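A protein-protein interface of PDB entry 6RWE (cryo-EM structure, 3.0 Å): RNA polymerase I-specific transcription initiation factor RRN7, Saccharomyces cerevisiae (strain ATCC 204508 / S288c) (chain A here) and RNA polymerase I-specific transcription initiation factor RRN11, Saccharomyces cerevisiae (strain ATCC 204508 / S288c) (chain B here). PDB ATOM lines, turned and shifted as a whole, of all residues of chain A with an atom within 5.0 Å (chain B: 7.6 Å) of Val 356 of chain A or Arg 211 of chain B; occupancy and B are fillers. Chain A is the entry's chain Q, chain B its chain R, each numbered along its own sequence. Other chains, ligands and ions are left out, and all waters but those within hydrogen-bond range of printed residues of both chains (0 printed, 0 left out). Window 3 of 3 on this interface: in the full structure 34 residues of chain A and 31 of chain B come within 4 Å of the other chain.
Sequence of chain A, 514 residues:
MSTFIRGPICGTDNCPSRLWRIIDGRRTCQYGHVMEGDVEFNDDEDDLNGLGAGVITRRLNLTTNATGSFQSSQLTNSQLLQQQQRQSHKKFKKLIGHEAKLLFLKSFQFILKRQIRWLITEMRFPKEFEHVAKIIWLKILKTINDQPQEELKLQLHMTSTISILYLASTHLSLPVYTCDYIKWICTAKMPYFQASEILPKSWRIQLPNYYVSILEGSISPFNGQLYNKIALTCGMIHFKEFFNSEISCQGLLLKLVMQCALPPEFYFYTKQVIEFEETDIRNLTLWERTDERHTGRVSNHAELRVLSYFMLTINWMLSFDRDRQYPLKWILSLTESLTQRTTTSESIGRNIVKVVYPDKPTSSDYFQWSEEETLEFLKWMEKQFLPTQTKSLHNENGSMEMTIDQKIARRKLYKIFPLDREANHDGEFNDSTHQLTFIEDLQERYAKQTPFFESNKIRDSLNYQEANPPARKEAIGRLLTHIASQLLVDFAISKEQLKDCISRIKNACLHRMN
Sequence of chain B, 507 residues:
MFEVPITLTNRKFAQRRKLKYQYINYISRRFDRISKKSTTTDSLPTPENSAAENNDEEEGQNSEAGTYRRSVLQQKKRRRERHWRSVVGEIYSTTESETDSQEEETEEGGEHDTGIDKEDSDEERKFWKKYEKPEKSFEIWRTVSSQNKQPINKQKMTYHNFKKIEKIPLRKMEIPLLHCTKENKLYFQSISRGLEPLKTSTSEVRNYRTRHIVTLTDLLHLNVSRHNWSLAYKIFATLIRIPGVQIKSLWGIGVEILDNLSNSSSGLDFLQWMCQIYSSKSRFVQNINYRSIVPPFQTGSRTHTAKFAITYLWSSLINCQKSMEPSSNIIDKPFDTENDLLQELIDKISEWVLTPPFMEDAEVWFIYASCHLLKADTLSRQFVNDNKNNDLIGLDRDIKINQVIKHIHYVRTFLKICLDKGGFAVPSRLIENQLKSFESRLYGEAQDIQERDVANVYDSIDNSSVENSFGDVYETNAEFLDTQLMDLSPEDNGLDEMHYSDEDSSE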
ATOM      1  N   CYS A 186      34.604 -10.685   0.471  1.00  0.00           N
ATOM      2  CA  CYS A 186      33.280 -10.416  -0.064  1.00  0.00           C
ATOM      3  C   CYS A 186      32.232 -10.350   1.033  1.00  0.00           C
ATOM      4  O   CYS A 186      31.206  -9.691   0.853  1.00  0.00           O
ATOM      5  CB  CYS A 186      32.902 -11.472  -1.097  1.00  0.00           C
ATOM      6  SG  CYS A 186      33.881 -11.393  -2.604  1.00  0.00           S
ATOM      7  N   SER A 220      35.917  -6.932  -6.888  1.00  0.00           N
ATOM      8  CA  SER A 220      36.697  -8.065  -6.325  1.00  0.00           C
ATOM      9  C   SER A 220      37.423  -8.843  -7.427  1.00  0.00           C
ATOM     10  O   SER A 220      36.917  -8.860  -8.551  1.00  0.00           O
ATOM     11  CB  SER A 220      35.868  -8.943  -5.443  1.00  0.00           C
ATOM     12  OG  SER A 220      35.191  -9.925  -6.202  1.00  0.00           O
ATOM     13  N   ILE A 352      26.912 -14.676  -0.728  1.00  0.00           N
ATOM     14  CA  ILE A 352      27.435 -13.331  -0.945  1.00  0.00           C
ATOM     15  C   ILE A 352      28.374 -13.323  -2.140  1.00  0.00           C
ATOM     16  O   ILE A 352      28.356 -12.399  -2.955  1.00  0.00           O
ATOM     17  CB  ILE A 352      28.164 -12.816   0.305  1.00  0.00           C
ATOM     18  CG1 ILE A 352      27.367 -13.089   1.574  1.00  0.00           C
ATOM     19  CG2 ILE A 352      28.399 -11.331   0.178  1.00  0.00           C
ATOM     20  CD1 ILE A 352      26.048 -12.420   1.649  1.00  0.00           C
ATOM     21  N   VAL A 353      29.194 -14.364  -2.269  1.00  0.00           N
ATOM     22  CA  VAL A 353      30.207 -14.381  -3.314  1.00  0.00           C
ATOM     23  C   VAL A 353      29.564 -14.691  -4.661  1.00  0.00           C
ATOM     24  O   VAL A 353      30.081 -14.300  -5.714  1.00  0.00           O
ATOM     25  CB  VAL A 353      31.305 -15.389  -2.926  1.00  0.00           C
ATOM     26  CG1 VAL A 353      32.508 -15.287  -3.843  1.00  0.00           C
ATOM     27  CG2 VAL A 353      31.713 -15.176  -1.488  1.00  0.00           C
ATOM     28  N   LYS A 354      28.411 -15.363  -4.650  1.00  0.00           N
ATOM     29  CA  LYS A 354      27.616 -15.492  -5.866  1.00  0.00           C
ATOM     30  C   LYS A 354      27.094 -14.142  -6.326  1.00  0.00           C
ATOM     31  O   LYS A 354      26.985 -13.896  -7.531  1.00  0.00           O
ATOM     32  CB  LYS A 354      26.444 -16.438  -5.625  1.00  0.00           C
ATOM     33  CG  LYS A 354      26.829 -17.869  -5.344  1.00  0.00           C
ATOM     34  CD  LYS A 354      25.596 -18.697  -5.073  1.00  0.00           C
ATOM     35  CE  LYS A 354      25.947 -20.122  -4.717  1.00  0.00           C
ATOM     36  NZ  LYS A 354      24.720 -20.900  -4.415  1.00  0.00           N
ATOM     37  N   VAL A 355      26.779 -13.260  -5.376  1.00  0.00           N
ATOM     38  CA  VAL A 355      26.213 -11.955  -5.692  1.00  0.00           C
ATOM     39  C   VAL A 355      27.254 -11.053  -6.345  1.00  0.00           C
ATOM     40  O   VAL A 355      26.964 -10.375  -7.339  1.00  0.00           O
ATOM     41  CB  VAL A 355      25.620 -11.333  -4.412  1.00  0.00           C
ATOM     42  CG1 VAL A 355      25.375  -9.860  -4.573  1.00  0.00           C
ATOM     43  CG2 VAL A 355      24.323 -12.023  -4.056  1.00  0.00           C
ATOM     44  N   VAL A 356      28.485 -11.064  -5.826  1.00  0.00           N
ATOM     45  CA  VAL A 356      29.501 -10.100  -6.236  1.00  0.00           C
ATOM     46  C   VAL A 356      29.960 -10.324  -7.673  1.00  0.00           C
ATOM     47  O   VAL A 356      30.273  -9.358  -8.376  1.00  0.00           O
ATOM     48  CB  VAL A 356      30.677 -10.154  -5.236  1.00  0.00           C
ATOM     49  CG1 VAL A 356      31.783  -9.162  -5.586  1.00  0.00           C
ATOM     50  CG2 VAL A 356      30.182  -9.878  -3.840  1.00  0.00           C
ATOM     51  N   TYR A 357      29.930 -11.560  -8.160  1.00  0.00           N
ATOM     52  CA  TYR A 357      30.476 -11.862  -9.472  1.00  0.00           C
ATOM     53  C   TYR A 357      29.388 -11.893 -10.531  1.00  0.00           C
ATOM     54  O   TYR A 357      28.547 -12.800 -10.512  1.00  0.00           O
ATOM     55  CB  TYR A 357      31.229 -13.184  -9.430  1.00  0.00           C
ATOM     56  CG  TYR A 357      32.526 -13.015  -8.697  1.00  0.00           C
ATOM     57  CD1 TYR A 357      33.622 -12.473  -9.341  1.00  0.00           C
ATOM     58  CD2 TYR A 357      32.642 -13.338  -7.358  1.00  0.00           C
ATOM     59  CE1 TYR A 357      34.803 -12.286  -8.683  1.00  0.00           C
ATOM     60  CE2 TYR A 357      33.828 -13.157  -6.687  1.00  0.00           C
ATOM     61  CZ  TYR A 357      34.906 -12.627  -7.359  1.00  0.00           C
ATOM     62  OH  TYR A 357      36.102 -12.435  -6.713  1.00  0.00           O
ATOM     63  N   PRO A 358      29.365 -10.935 -11.468  1.00  0.00           N
ATOM     64  CA  PRO A 358      28.254 -10.852 -12.421  1.00  0.00           C
ATOM     65  C   PRO A 358      28.450 -11.669 -13.685  1.00  0.00           C
ATOM     66  O   PRO A 358      27.471 -11.994 -14.363  1.00  0.00           O
ATOM     67  CB  PRO A 358      28.214  -9.358 -12.750  1.00  0.00           C
ATOM     68  CG  PRO A 358      29.634  -8.935 -12.649  1.00  0.00           C
ATOM     69  CD  PRO A 358      30.254  -9.763 -11.561  1.00  0.00           C
ATOM     70  N   ILE B   6      20.552   3.946  -9.629  1.00  0.00           N
ATOM     71  CA  ILE B   6      21.977   4.233  -9.595  1.00  0.00           C
ATOM     72  C   ILE B   6      22.301   5.190 -10.730  1.00  0.00           C
ATOM     73  O   ILE B   6      21.913   4.953 -11.877  1.00  0.00           O
ATOM     74  CB  ILE B   6      22.825   2.951  -9.716  1.00  0.00           C
ATOM     75  CG1 ILE B   6      22.569   2.012  -8.545  1.00  0.00           C
ATOM     76  CG2 ILE B   6      24.304   3.273  -9.744  1.00  0.00           C
ATOM     77  CD1 ILE B   6      23.163   0.658  -8.755  1.00  0.00           C
ATOM     78  N   THR B 202      23.629  -2.240 -17.214  1.00  0.00           N
ATOM     79  CA  THR B 202      23.770  -2.383 -15.774  1.00  0.00           C
ATOM     80  C   THR B 202      24.324  -3.734 -15.356  1.00  0.00           C
ATOM     81  O   THR B 202      24.650  -3.911 -14.179  1.00  0.00           O
ATOM     82  CB  THR B 202      22.416  -2.190 -15.092  1.00  0.00           C
ATOM     83  OG1 THR B 202      21.550  -3.270 -15.457  1.00  0.00           O
ATOM     84  CG2 THR B 202      21.781  -0.905 -15.552  1.00  0.00           C
ATOM     85  N   SER B 203      24.440  -4.687 -16.277  1.00  0.00           N
ATOM     86  CA  SER B 203      24.689  -6.071 -15.896  1.00  0.00           C
ATOM     87  C   SER B 203      26.146  -6.372 -15.567  1.00  0.00           C
ATOM     88  O   SER B 203      26.433  -7.484 -15.114  1.00  0.00           O
ATOM     89  CB  SER B 203      24.226  -7.008 -17.009  1.00  0.00           C
ATOM     90  OG  SER B 203      24.486  -8.357 -16.668  1.00  0.00           O
ATOM     91  N   GLU B 204      27.082  -5.482 -15.887  1.00  0.00           N
ATOM     92  CA  GLU B 204      28.497  -5.763 -15.529  1.00  0.00           C
ATOM     93  C   GLU B 204      29.049  -4.604 -14.704  1.00  0.00           C
ATOM     94  O   GLU B 204      30.211  -4.241 -14.904  1.00  0.00           O
ATOM     95  CB  GLU B 204      29.373  -5.902 -16.766  1.00  0.00           C
ATOM     96  CG  GLU B 204      29.341  -4.661 -17.615  1.00  0.00           C
ATOM     97  CD  GLU B 204      28.138  -4.741 -18.518  1.00  0.00           C
ATOM     98  OE1 GLU B 204      27.096  -5.193 -18.028  1.00  0.00           O
ATOM     99  OE2 GLU B 204      28.268  -4.417 -19.710  1.00  0.00           O
ATOM    100  N   VAL B 205      28.236  -4.018 -13.834  1.00  0.00           N
ATOM    101  CA  VAL B 205      28.745  -2.848 -13.074  1.00  0.00           C
ATOM    102  C   VAL B 205      29.952  -3.301 -12.243  1.00  0.00           C
ATOM    103  O   VAL B 205      30.967  -2.597 -12.286  1.00  0.00           O
ATOM    104  CB  VAL B 205      27.611  -2.204 -12.252  1.00  0.00           C
ATOM    105  CG1 VAL B 205      26.890  -3.186 -11.353  1.00  0.00           C
ATOM    106  CG2 VAL B 205      28.049  -0.979 -11.475  1.00  0.00           C
ATOM    107  N   ARG B 206      29.826  -4.443 -11.566  1.00  0.00           N
ATOM    108  CA  ARG B 206      30.899  -5.018 -10.714  1.00  0.00           C
ATOM    109  C   ARG B 206      31.658  -3.939  -9.933  1.00  0.00           C
ATOM    110  O   ARG B 206      32.828  -3.711 -10.248  1.00  0.00           O
ATOM    111  CB  ARG B 206      31.840  -5.909 -11.530  1.00  0.00           C
ATOM    112  CG  ARG B 206      32.720  -5.168 -12.523  1.00  0.00           C
ATOM    113  CD  ARG B 206      33.679  -6.118 -13.217  1.00  0.00           C
ATOM    114  NE  ARG B 206      33.700  -7.437 -12.606  1.00  0.00           N
ATOM    115  CZ  ARG B 206      33.500  -8.574 -13.258  1.00  0.00           C
ATOM    116  NH1 ARG B 206      33.266  -8.557 -14.558  1.00  0.00           N
ATOM    117  NH2 ARG B 206      33.536  -9.722 -12.609  1.00  0.00           N
ATOM    118  N   ASN B 207      30.986  -3.287  -8.981  1.00  0.00           N
ATOM    119  CA  ASN B 207      31.599  -2.345  -8.059  1.00  0.00           C
ATOM    120  C   ASN B 207      31.447  -2.758  -6.600  1.00  0.00           C
ATOM    121  O   ASN B 207      31.895  -2.014  -5.719  1.00  0.00           O
ATOM    122  CB  ASN B 207      30.998  -0.943  -8.265  1.00  0.00           C
ATOM    123  CG  ASN B 207      31.915   0.185  -7.806  1.00  0.00           C
ATOM    124  OD1 ASN B 207      33.032  -0.044  -7.349  1.00  0.00           O
ATOM    125  ND2 ASN B 207      31.439   1.415  -7.933  1.00  0.00           N
ATOM    126  N   TYR B 208      30.750  -3.867  -6.316  1.00  0.00           N
ATOM    127  CA  TYR B 208      30.509  -4.502  -5.010  1.00  0.00           C
ATOM    128  C   TYR B 208      29.566  -3.696  -4.114  1.00  0.00           C
ATOM    129  O   TYR B 208      28.927  -4.255  -3.218  1.00  0.00           O
ATOM    130  CB  TYR B 208      31.837  -4.779  -4.277  1.00  0.00           C
ATOM    131  CG  TYR B 208      31.702  -5.354  -2.884  1.00  0.00           C
ATOM    132  CD1 TYR B 208      31.438  -6.695  -2.690  1.00  0.00           C
ATOM    133  CD2 TYR B 208      31.814  -4.543  -1.765  1.00  0.00           C
ATOM    134  CE1 TYR B 208      31.313  -7.218  -1.424  1.00  0.00           C
ATOM    135  CE2 TYR B 208      31.674  -5.054  -0.499  1.00  0.00           C
ATOM    136  CZ  TYR B 208      31.422  -6.392  -0.333  1.00  0.00           C
ATOM    137  OH  TYR B 208      31.287  -6.914   0.931  1.00  0.00           O
ATOM    138  N   ARG B 209      29.367  -2.421  -4.420  1.00  0.00           N
ATOM    139  CA  ARG B 209      28.376  -1.589  -3.767  1.00  0.00           C
ATOM    140  C   ARG B 209      27.135  -1.481  -4.631  1.00  0.00           C
ATOM    141  O   ARG B 209      26.030  -1.789  -4.181  1.00  0.00           O
ATOM    142  CB  ARG B 209      28.958  -0.205  -3.493  1.00  0.00           C
ATOM    143  CG  ARG B 209      28.040   0.743  -2.775  1.00  0.00           C
ATOM    144  CD  ARG B 209      28.743   2.062  -2.616  1.00  0.00           C
ATOM    145  NE  ARG B 209      29.006   2.651  -3.923  1.00  0.00           N
ATOM    146  CZ  ARG B 209      29.811   3.685  -4.137  1.00  0.00           C
ATOM    147  NH1 ARG B 209      29.981   4.144  -5.367  1.00  0.00           N
ATOM    148  NH2 ARG B 209      30.451   4.254  -3.125  1.00  0.00           N
ATOM    149  N   THR B 210      27.327  -1.088  -5.890  1.00  0.00           N
ATOM    150  CA  THR B 210      26.263  -1.154  -6.880  1.00  0.00           C
ATOM    151  C   THR B 210      25.839  -2.586  -7.141  1.00  0.00           C
ATOM    152  O   THR B 210      24.677  -2.835  -7.462  1.00  0.00           O
ATOM    153  CB  THR B 210      26.730  -0.524  -8.178  1.00  0.00           C
ATOM    154  OG1 THR B 210      27.772  -1.329  -8.721  1.00  0.00           O
ATOM    155  CG2 THR B 210      27.283   0.853  -7.909  1.00  0.00           C
ATOM    156  N   ARG B 211      26.760  -3.531  -6.990  1.00  0.00           N
ATOM    157  CA  ARG B 211      26.458  -4.939  -7.200  1.00  0.00           C
ATOM    158  C   ARG B 211      25.530  -5.475  -6.119  1.00  0.00           C
ATOM    159  O   ARG B 211      24.796  -6.439  -6.354  1.00  0.00           O
ATOM    160  CB  ARG B 211      27.771  -5.712  -7.245  1.00  0.00           C
ATOM    161  CG  ARG B 211      27.711  -7.167  -7.614  1.00  0.00           C
ATOM    162  CD  ARG B 211      27.345  -7.356  -9.063  1.00  0.00           C
ATOM    163  NE  ARG B 211      25.956  -7.753  -9.235  1.00  0.00           N
ATOM    164  CZ  ARG B 211      25.314  -7.724 -10.395  1.00  0.00           C
ATOM    165  NH1 ARG B 211      25.923  -7.268 -11.477  1.00  0.00           N
ATOM    166  NH2 ARG B 211      24.054  -8.121 -10.469  1.00  0.00           N
ATOM    167  N   HIS B 212      25.530  -4.857  -4.944  1.00  0.00           N
ATOM    168  CA  HIS B 212      24.543  -5.172  -3.926  1.00  0.00           C
ATOM    169  C   HIS B 212      23.260  -4.379  -4.071  1.00  0.00           C
ATOM    170  O   HIS B 212      22.217  -4.838  -3.594  1.00  0.00           O
ATOM    171  CB  HIS B 212      25.116  -4.932  -2.535  1.00  0.00           C
ATOM    172  CG  HIS B 212      26.066  -5.993  -2.100  1.00  0.00           C
ATOM    173  ND1 HIS B 212      27.383  -6.018  -2.497  1.00  0.00           N
ATOM    174  CD2 HIS B 212      25.892  -7.065  -1.295  1.00  0.00           C
ATOM    175  CE1 HIS B 212      27.977  -7.068  -1.963  1.00  0.00           C
ATOM    176  NE2 HIS B 212      27.097  -7.716  -1.224  1.00  0.00           N
ATOM    177  N   ILE B 213      23.310  -3.201  -4.691  1.00  0.00           N
ATOM    178  CA  ILE B 213      22.082  -2.466  -4.956  1.00  0.00           C
ATOM    179  C   ILE B 213      21.229  -3.216  -5.967  1.00  0.00           C
ATOM    180  O   ILE B 213      20.013  -3.343  -5.792  1.00  0.00           O
ATOM    181  CB  ILE B 213      22.407  -1.042  -5.433  1.00  0.00           C
ATOM    182  CG1 ILE B 213      23.153  -0.276  -4.351  1.00  0.00           C
ATOM    183  CG2 ILE B 213      21.142  -0.292  -5.775  1.00  0.00           C
ATOM    184  CD1 ILE B 213      23.735   1.020  -4.841  1.00  0.00           C
ATOM    185  N   VAL B 214      21.865  -3.767  -7.008  1.00  0.00           N
ATOM    186  CA  VAL B 214      21.169  -4.542  -8.032  1.00  0.00           C
ATOM    187  C   VAL B 214      20.520  -5.778  -7.427  1.00  0.00           C
ATOM    188  O   VAL B 214      19.407  -6.158  -7.808  1.00  0.00           O
ATOM    189  CB  VAL B 214      22.155  -4.895  -9.166  1.00  0.00           C
ATOM    190  CG1 VAL B 214      21.530  -5.814 -10.191  1.00  0.00           C
ATOM    191  CG2 VAL B 214      22.622  -3.639  -9.857  1.00  0.00           C
ATOM    192  N   THR B 215      21.154  -6.376  -6.425  1.00  0.00           N
ATOM    193  CA  THR B 215      20.521  -7.481  -5.722  1.00  0.00           C
ATOM    194  C   THR B 215      19.396  -6.987  -4.824  1.00  0.00           C
ATOM    195  O   THR B 215      18.299  -7.553  -4.823  1.00  0.00           O
ATOM    196  CB  THR B 215      21.562  -8.245  -4.915  1.00  0.00           C
ATOM    197  OG1 THR B 215      22.560  -8.744  -5.808  1.00  0.00           O
ATOM    198  CG2 THR B 215      20.925  -9.412  -4.190  1.00  0.00           C
ATOM    199  N   LEU B 216      19.634  -5.910  -4.081  1.00  0.00           N
ATOM    200  CA  LEU B 216      18.642  -5.440  -3.126  1.00  0.00           C
ATOM    201  C   LEU B 216      17.446  -4.751  -3.761  1.00  0.00           C
ATOM    202  O   LEU B 216      16.442  -4.558  -3.071  1.00  0.00           O
ATOM    203  CB  LEU B 216      19.272  -4.487  -2.121  1.00  0.00           C
ATOM    204  CG  LEU B 216      20.133  -5.123  -1.050  1.00  0.00           C
ATOM    205  CD1 LEU B 216      20.797  -4.033  -0.274  1.00  0.00           C
ATOM    206  CD2 LEU B 216      19.253  -5.940  -0.153  1.00  0.00           C
ATOM    207  N   ASP B 218      16.165  -5.965  -6.912  1.00  0.00           N
ATOM    208  CA  ASP B 218      15.447  -7.120  -7.430  1.00  0.00           C
ATOM    209  C   ASP B 218      14.844  -7.948  -6.307  1.00  0.00           C
ATOM    210  O   ASP B 218      13.800  -8.573  -6.498  1.00  0.00           O
ATOM    211  CB  ASP B 218      16.364  -7.975  -8.295  1.00  0.00           C
ATOM    212  CG  ASP B 218      16.677  -7.329  -9.626  1.00  0.00           C
ATOM    213  OD1 ASP B 218      15.859  -6.515 -10.088  1.00  0.00           O
ATOM    214  OD2 ASP B 218      17.721  -7.649 -10.227  1.00  0.00           O
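The side-chain hydroxyl (OH) of Tyr 208 of chain B lies within hydrogen-bond range of the backbone carbonyl oxygen (O) of Cys 186 of chain A (2.8 Å).
NE of Arg 211 of chain B sits close to O of Val 355 of chain A, at 3.4 Å.
The backbone carbonyl oxygen of Tyr 208 of chain B sits at hydrogen-bond distance from a ring nitrogen (ND1) of His 212 of chain B, at 2.5 Å.
O of Arg 211 of chain B is in hydrogen-bond range of OG1 of Thr 215 of chain B (3.3 Å).
Among the printed residues, merely in contact across the chains: Val 355 of chain A with Thr 215 of chain B (3.3 Å), Pro 358 of chain A with Arg 211 of chain B (3.4 Å), Pro 358 of chain A with Arg 206 of chain B (3.4 Å), Val 356 of chain A with Arg 211 of chain B (3.5 Å), Pro 358 of chain A with Ser 203 of chain B (3.5 Å) and Val 356 of chain A with Tyr 208 of chain B (3.6 Å).
Of the printed residues of chain B, Cys 186 of chain A touches Tyr 208 (2.8 Å).
Of the printed residues of chain B, Pro 358 of chain A touches Ser 203, Arg 206 and Arg 211.
Glu 204 of chain B touches none of the printed residues of chain A.
Of the printed residues of chain A, Tyr 208 of chain B touches Cys 186 (2.8 Å) and Val 356 (3.6 Å).
Arg 211 of chain B touches three residues of chain A.
Printed residues of chain A within 4 Å of Thr 215 of chain B: Val 355 (3.3 Å).
The nearest residue of chain B that does not touch Val 356 of chain A is His 212 of chain B (4.04 Å).
The nearest printed residue of chain A that does not touch Thr 215 of chain B is Val 356 of chain A (6.4 Å).
Hydrophobic or aromatic side chains of chain A that line the printed part of chain B: Val 355, Val 356 and Pro 358.
Along chain A the printed residues that touch a printed residue of chain B span positions 186 to 358.
Printed residues of chain B that touch a printed residue of chain A: Ser 203, Arg 206, Tyr 208, Arg 211 and Thr 215.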
